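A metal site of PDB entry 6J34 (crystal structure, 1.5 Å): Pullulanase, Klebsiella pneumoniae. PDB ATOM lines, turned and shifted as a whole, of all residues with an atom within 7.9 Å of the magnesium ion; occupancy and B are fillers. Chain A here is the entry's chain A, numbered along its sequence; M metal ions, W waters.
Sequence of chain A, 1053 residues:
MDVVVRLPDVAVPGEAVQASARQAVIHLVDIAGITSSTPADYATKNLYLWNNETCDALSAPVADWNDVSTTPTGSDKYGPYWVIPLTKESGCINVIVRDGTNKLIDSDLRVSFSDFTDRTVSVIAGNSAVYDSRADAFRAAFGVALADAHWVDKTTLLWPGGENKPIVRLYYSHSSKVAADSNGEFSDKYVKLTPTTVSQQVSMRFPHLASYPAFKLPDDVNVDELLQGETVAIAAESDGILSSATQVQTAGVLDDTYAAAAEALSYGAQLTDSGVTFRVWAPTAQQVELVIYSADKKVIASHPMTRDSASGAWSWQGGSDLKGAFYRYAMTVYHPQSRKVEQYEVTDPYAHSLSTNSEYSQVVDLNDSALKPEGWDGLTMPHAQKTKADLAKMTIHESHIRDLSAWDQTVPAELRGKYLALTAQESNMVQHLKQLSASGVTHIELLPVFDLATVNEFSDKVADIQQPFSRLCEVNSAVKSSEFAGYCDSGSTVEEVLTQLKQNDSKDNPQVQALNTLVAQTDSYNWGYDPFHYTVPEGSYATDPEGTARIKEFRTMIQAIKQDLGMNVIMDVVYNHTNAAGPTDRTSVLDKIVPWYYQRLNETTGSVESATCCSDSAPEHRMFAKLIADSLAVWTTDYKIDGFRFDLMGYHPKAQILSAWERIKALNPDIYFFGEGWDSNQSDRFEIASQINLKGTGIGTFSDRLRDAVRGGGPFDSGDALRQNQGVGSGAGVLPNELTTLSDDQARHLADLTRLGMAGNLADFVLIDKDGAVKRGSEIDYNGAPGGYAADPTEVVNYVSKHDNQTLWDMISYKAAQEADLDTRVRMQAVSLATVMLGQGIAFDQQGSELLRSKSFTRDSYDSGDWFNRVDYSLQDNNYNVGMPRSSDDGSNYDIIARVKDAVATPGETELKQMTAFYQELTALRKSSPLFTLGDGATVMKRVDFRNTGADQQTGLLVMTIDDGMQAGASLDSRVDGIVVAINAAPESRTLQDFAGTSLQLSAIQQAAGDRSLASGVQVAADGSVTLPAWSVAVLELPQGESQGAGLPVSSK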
ATOM      1  N   SER A 929     -17.239  33.738 -11.060  1.00  0.00           N
ATOM      2  CA  SER A 929     -16.419  32.596 -11.484  1.00  0.00           C
ATOM      3  C   SER A 929     -16.532  32.368 -12.978  1.00  0.00           C
ATOM      4  O   SER A 929     -17.650  32.376 -13.526  1.00  0.00           O
ATOM      5  CB  SER A 929     -16.836  31.304 -10.760  1.00  0.00           C
ATOM      6  OG  SER A 929     -16.128  30.183 -11.265  1.00  0.00           O
ATOM      7  N   LEU A 931     -16.383  29.586 -14.274  1.00  0.00           N
ATOM      8  CA  LEU A 931     -17.040  28.293 -14.475  1.00  0.00           C
ATOM      9  C   LEU A 931     -18.504  28.453 -14.910  1.00  0.00           C
ATOM     10  O   LEU A 931     -19.046  27.555 -15.563  1.00  0.00           O
ATOM     11  CB  LEU A 931     -16.948  27.456 -13.206  1.00  0.00           C
ATOM     12  CG  LEU A 931     -15.533  27.008 -12.838  1.00  0.00           C
ATOM     13  CD1 LEU A 931     -15.542  26.303 -11.502  1.00  0.00           C
ATOM     14  CD2 LEU A 931     -14.973  26.099 -13.904  1.00  0.00           C
ATOM     15  N   ARG A 943     -17.378  19.548 -18.742  1.00  0.00           N
ATOM     16  CA  ARG A 943     -17.423  20.021 -17.360  1.00  0.00           C
ATOM     17  C   ARG A 943     -18.805  20.004 -16.694  1.00  0.00           C
ATOM     18  O   ARG A 943     -18.872  19.935 -15.471  1.00  0.00           O
ATOM     19  CB  ARG A 943     -16.845  21.452 -17.269  1.00  0.00           C
ATOM     20  CG  ARG A 943     -15.354  21.502 -17.629  1.00  0.00           C
ATOM     21  CD  ARG A 943     -14.816  22.928 -17.575  1.00  0.00           C
ATOM     22  NE  ARG A 943     -13.379  23.019 -17.909  1.00  0.00           N
ATOM     23  CZ  ARG A 943     -12.415  23.276 -17.027  1.00  0.00           C
ATOM     24  NH1 ARG A 943     -12.714  23.454 -15.738  1.00  0.00           N
ATOM     25  NH2 ARG A 943     -11.151  23.362 -17.439  1.00  0.00           N
ATOM     26  N   ASP A 963     -17.424  21.176 -13.344  1.00  0.00           N
ATOM     27  CA  ASP A 963     -16.158  20.609 -12.906  1.00  0.00           C
ATOM     28  C   ASP A 963     -14.996  21.584 -13.154  1.00  0.00           C
ATOM     29  O   ASP A 963     -14.882  22.168 -14.240  1.00  0.00           O
ATOM     30  CB  ASP A 963     -15.904  19.311 -13.686  1.00  0.00           C
ATOM     31  CG  ASP A 963     -14.765  18.514 -13.129  1.00  0.00           C
ATOM     32  OD1 ASP A 963     -14.386  18.721 -11.951  1.00  0.00           O
ATOM     33  OD2 ASP A 963     -14.247  17.661 -13.880  1.00  0.00           O
ATOM     34  N   ASP A 964     -14.145  21.759 -12.138  1.00  0.00           N
ATOM     35  CA  ASP A 964     -12.844  22.412 -12.309  1.00  0.00           C
ATOM     36  C   ASP A 964     -11.694  21.494 -11.900  1.00  0.00           C
ATOM     37  O   ASP A 964     -10.557  21.963 -11.735  1.00  0.00           O
ATOM     38  CB  ASP A 964     -12.759  23.740 -11.548  1.00  0.00           C
ATOM     39  CG  ASP A 964     -11.771  24.735 -12.192  1.00  0.00           C
ATOM     40  OD1 ASP A 964     -11.677  24.761 -13.443  1.00  0.00           O
ATOM     41  OD2 ASP A 964     -11.093  25.484 -11.449  1.00  0.00           O
ATOM     42  N   GLY A 965     -11.969  20.193 -11.752  1.00  0.00           N
ATOM     43  CA  GLY A 965     -10.983  19.250 -11.298  1.00  0.00           C
ATOM     44  C   GLY A 965     -10.123  18.678 -12.418  1.00  0.00           C
ATOM     45  O   GLY A 965     -10.240  19.035 -13.593  1.00  0.00           O
ATOM     46  N   ALA A 970      -7.455  22.152 -17.254  1.00  0.00           N
ATOM     47  CA  ALA A 970      -6.862  23.142 -16.381  1.00  0.00           C
ATOM     48  C   ALA A 970      -7.875  23.685 -15.389  1.00  0.00           C
ATOM     49  O   ALA A 970      -9.087  23.695 -15.641  1.00  0.00           O
ATOM     50  CB  ALA A 970      -6.300  24.305 -17.206  1.00  0.00           C
ATOM     51  N   SER A 971      -7.381  24.127 -14.239  1.00  0.00           N
ATOM     52  CA  SER A 971      -8.226  24.881 -13.312  1.00  0.00           C
ATOM     53  C   SER A 971      -8.429  26.280 -13.896  1.00  0.00           C
ATOM     54  O   SER A 971      -7.457  26.992 -14.149  1.00  0.00           O
ATOM     55  CB  SER A 971      -7.539  24.967 -11.949  1.00  0.00           C
ATOM     56  OG  SER A 971      -8.190  25.880 -11.073  1.00  0.00           O
ATOM     57  N   LEU A 972      -9.691  26.626 -14.162  1.00  0.00           N
ATOM     58  CA  LEU A 972     -10.035  27.950 -14.654  1.00  0.00           C
ATOM     59  C   LEU A 972     -10.264  28.939 -13.521  1.00  0.00           C
ATOM     60  O   LEU A 972     -10.248  30.157 -13.744  1.00  0.00           O
ATOM     61  CB  LEU A 972     -11.288  27.889 -15.520  1.00  0.00           C
ATOM     62  CG  LEU A 972     -11.250  26.935 -16.726  1.00  0.00           C
ATOM     63  CD1 LEU A 972     -12.617  26.841 -17.378  1.00  0.00           C
ATOM     64  CD2 LEU A 972     -10.196  27.379 -17.734  1.00  0.00           C
ATOM     65  N   ASP A 973     -10.470  28.435 -12.302  1.00  0.00           N
ATOM     66  CA  ASP A 973     -10.763  29.250 -11.146  1.00  0.00           C
ATOM     67  C   ASP A 973      -9.857  28.769 -10.028  1.00  0.00           C
ATOM     68  O   ASP A 973      -9.966  27.609  -9.603  1.00  0.00           O
ATOM     69  CB  ASP A 973     -12.245  29.103 -10.785  1.00  0.00           C
ATOM     70  CG  ASP A 973     -12.710  30.053  -9.703  1.00  0.00           C
ATOM     71  OD1 ASP A 973     -11.889  30.517  -8.884  1.00  0.00           O
ATOM     72  OD2 ASP A 973     -13.931  30.323  -9.654  1.00  0.00           O
ATOM     73  N   SER A 974      -8.955  29.634  -9.565  1.00  0.00           N
ATOM     74  CA  SER A 974      -8.000  29.216  -8.550  1.00  0.00           C
ATOM     75  C   SER A 974      -8.638  29.006  -7.190  1.00  0.00           C
ATOM     76  O   SER A 974      -8.013  28.383  -6.309  1.00  0.00           O
ATOM     77  CB  SER A 974      -6.877  30.245  -8.401  1.00  0.00           C
ATOM     78  OG  SER A 974      -7.387  31.477  -7.929  1.00  0.00           O
ATOM     79  N   ARG A 975      -9.851  29.505  -6.983  1.00  0.00           N
ATOM     80  CA  ARG A 975     -10.480  29.393  -5.677  1.00  0.00           C
ATOM     81  C   ARG A 975     -11.278  28.125  -5.498  1.00  0.00           C
ATOM     82  O   ARG A 975     -11.540  27.725  -4.353  1.00  0.00           O
ATOM     83  CB  ARG A 975     -11.383  30.606  -5.420  1.00  0.00           C
ATOM     84  CG  ARG A 975     -10.634  31.926  -5.423  1.00  0.00           C
ATOM     85  CD  ARG A 975     -11.508  33.062  -4.886  1.00  0.00           C
ATOM     86  NE  ARG A 975     -10.832  34.354  -4.956  1.00  0.00           N
ATOM     87  CZ  ARG A 975     -11.333  35.489  -4.481  1.00  0.00           C
ATOM     88  NH1 ARG A 975     -12.535  35.498  -3.894  1.00  0.00           N
ATOM     89  NH2 ARG A 975     -10.648  36.621  -4.582  1.00  0.00           N
ATOM     90  N   VAL A 976     -11.707  27.464  -6.577  1.00  0.00           N
ATOM     91  CA  VAL A 976     -12.588  26.306  -6.480  1.00  0.00           C
ATOM     92  C   VAL A 976     -12.152  25.197  -7.421  1.00  0.00           C
ATOM     93  O   VAL A 976     -11.567  25.438  -8.483  1.00  0.00           O
ATOM     94  CB  VAL A 976     -14.072  26.669  -6.740  1.00  0.00           C
ATOM     95  CG1 VAL A 976     -14.548  27.735  -5.788  1.00  0.00           C
ATOM     96  CG2 VAL A 976     -14.269  27.112  -8.197  1.00  0.00           C
ATOM     97  N   ASP A 977     -12.472  23.956  -7.022  1.00  0.00           N
ATOM     98  CA  ASP A 977     -12.347  22.780  -7.862  1.00  0.00           C
ATOM     99  C   ASP A 977     -13.657  22.362  -8.516  1.00  0.00           C
ATOM    100  O   ASP A 977     -13.683  21.404  -9.287  1.00  0.00           O
ATOM    101  CB  ASP A 977     -11.854  21.579  -7.030  1.00  0.00           C
ATOM    102  CG  ASP A 977     -10.369  21.644  -6.696  1.00  0.00           C
ATOM    103  OD1 ASP A 977      -9.562  22.132  -7.525  1.00  0.00           O
ATOM    104  OD2 ASP A 977     -10.018  21.171  -5.594  1.00  0.00           O
ATOM    105  N   GLY A 978     -14.751  23.056  -8.207  1.00  0.00           N
ATOM    106  CA  GLY A 978     -16.042  22.699  -8.763  1.00  0.00           C
ATOM    107  C   GLY A 978     -17.142  23.534  -8.145  1.00  0.00           C
ATOM    108  O   GLY A 978     -16.967  24.086  -7.059  1.00  0.00           O
ATOM    109  N   LEU A1038     -16.488  23.504  -4.146  1.00  0.00           N
ATOM    110  CA  LEU A1038     -15.415  22.722  -3.581  1.00  0.00           C
ATOM    111  C   LEU A1038     -14.210  23.635  -3.444  1.00  0.00           C
ATOM    112  O   LEU A1038     -13.666  24.067  -4.465  1.00  0.00           O
ATOM    113  CB  LEU A1038     -15.080  21.543  -4.491  1.00  0.00           C
ATOM    114  CG  LEU A1038     -16.140  20.453  -4.658  1.00  0.00           C
ATOM    115  CD1 LEU A1038     -15.658  19.400  -5.627  1.00  0.00           C
ATOM    116  CD2 LEU A1038     -16.519  19.826  -3.325  1.00  0.00           C
ATOM    117  N   PRO A1039     -13.766  23.968  -2.236  1.00  0.00           N
ATOM    118  CA  PRO A1039     -12.617  24.876  -2.102  1.00  0.00           C
ATOM    119  C   PRO A1039     -11.359  24.233  -2.658  1.00  0.00           C
ATOM    120  O   PRO A1039     -11.087  23.053  -2.438  1.00  0.00           O
ATOM    121  CB  PRO A1039     -12.488  25.073  -0.584  1.00  0.00           C
ATOM    122  CG  PRO A1039     -13.578  24.281   0.057  1.00  0.00           C
ATOM    123  CD  PRO A1039     -14.210  23.387  -0.953  1.00  0.00           C
ATOM    124  N   GLN A1040     -10.564  25.029  -3.372  1.00  0.00           N
ATOM    125  CA  GLN A1040      -9.324  24.527  -3.971  1.00  0.00           C
ATOM    126  C   GLN A1040      -8.179  24.699  -2.997  1.00  0.00           C
ATOM    127  O   GLN A1040      -8.027  25.764  -2.378  1.00  0.00           O
ATOM    128  CB  GLN A1040      -9.021  25.259  -5.276  1.00  0.00           C
ATOM    129  CG  GLN A1040      -7.804  24.698  -6.020  1.00  0.00           C
ATOM    130  CD  GLN A1040      -7.787  25.135  -7.466  1.00  0.00           C
ATOM    131  OE1 GLN A1040      -8.831  25.506  -8.017  1.00  0.00           O
ATOM    132  NE2 GLN A1040      -6.623  25.097  -8.089  1.00  0.00           N
ATOM    133  N   GLY A1041      -7.375  23.655  -2.852  1.00  0.00           N
ATOM    134  CA  GLY A1041      -6.240  23.676  -1.962  1.00  0.00           C
ATOM    135  C   GLY A1041      -4.936  23.886  -2.698  1.00  0.00           C
ATOM    136  O   GLY A1041      -4.869  24.624  -3.691  1.00  0.00           O
ATOM    137  N   SER A1043      -3.096  22.091  -4.650  1.00  0.00           N
ATOM    138  CA  SER A1043      -3.121  21.697  -6.037  1.00  0.00           C
ATOM    139  C   SER A1043      -4.528  21.472  -6.509  1.00  0.00           C
ATOM    140  O   SER A1043      -5.415  21.272  -5.723  1.00  0.00           O
ATOM    141  CB  SER A1043      -2.430  20.357  -6.216  1.00  0.00           C
ATOM    142  OG  SER A1043      -1.145  20.404  -5.707  1.00  0.00           O
ATOM    143  N   GLN A1044      -4.730  21.503  -7.815  1.00  0.00           N
ATOM    144  CA  GLN A1044      -6.029  21.159  -8.371  1.00  0.00           C
ATOM    145  C   GLN A1044      -6.489  19.810  -7.838  1.00  0.00           C
ATOM    146  O   GLN A1044      -5.711  18.856  -7.754  1.00  0.00           O
ATOM    147  CB  GLN A1044      -5.914  21.098  -9.891  1.00  0.00           C
ATOM    148  CG  GLN A1044      -7.201  20.780 -10.615  1.00  0.00           C
ATOM    149  CD  GLN A1044      -6.990  20.745 -12.107  1.00  0.00           C
ATOM    150  OE1 GLN A1044      -5.905  20.400 -12.584  1.00  0.00           O
ATOM    151  NE2 GLN A1044      -8.023  21.104 -12.859  1.00  0.00           N
ATOM    152  N   GLY A1045      -7.760  19.743  -7.450  1.00  0.00           N
ATOM    153  CA  GLY A1045      -8.323  18.559  -6.839  1.00  0.00           C
ATOM    154  C   GLY A1045      -9.154  17.718  -7.797  1.00  0.00           C
ATOM    155  O   GLY A1045      -9.140  17.914  -9.014  1.00  0.00           O
HETATM  156 MG    MG M   1      -9.957  25.618  -9.769  1.00  0.00          MG
HETATM  157  O   HOH W   1      -9.592  23.608  -9.785  1.00  0.00           O
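The side-chain amide oxygen (OE1) of Gln 1040 sits close to the side-chain carboxylate (OD1) of Asp 977, 3.5 Å away. The side-chain hydroxyl of Ser 929 is in hydrogen-bond range of the side-chain carboxylate of Asp 973. The backbone NH of Leu 972 lies within hydrogen-bond range of the side-chain carboxylate of Asp 964. The side-chain amide oxygen (OE1) of Gln 1040 lies close to the backbone carbonyl oxygen (O) of Ser 974, at 3.4 Å. The side-chain carboxylate (OD1) of Asp 973 sits at hydrogen-bond distance from the backbone NH (N) of Arg 975. The backbone carbonyl oxygen (O) of Arg 975 is in hydrogen-bond range of the backbone NH (N) of Gln 1040. The backbone carbonyl oxygen of Asp 977 sits at hydrogen-bond distance from the backbone NH of Asp 964, at 2.9 Å. OD1 of Asp 964 lies within salt-bridge range of NH1 of Arg 943.
Of the 22 residues printed, 5 come within 4 Å of the magnesium ion.
O of Asp 973 binds the magnesium ion (2.0 Å). The magnesium ion is bound by OD2 of Asp 964. The magnesium ion is bound by water W1 (2.0 Å). The backbone carbonyl oxygen (O) of Val 976 is bound to the magnesium ion (2.1 Å). The magnesium ion is bound by the side-chain amide oxygen (OE1) of Gln 1040. The side-chain hydroxyl (OG) of Ser 971 binds the magnesium ion (2.2 Å). The magnesium ion has six donor atoms within binding distance.
Water W1 lies within hydrogen-bond range of OD1 of Asp 977 (2.7 Å) and O of Asp 964 (2.7 Å).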
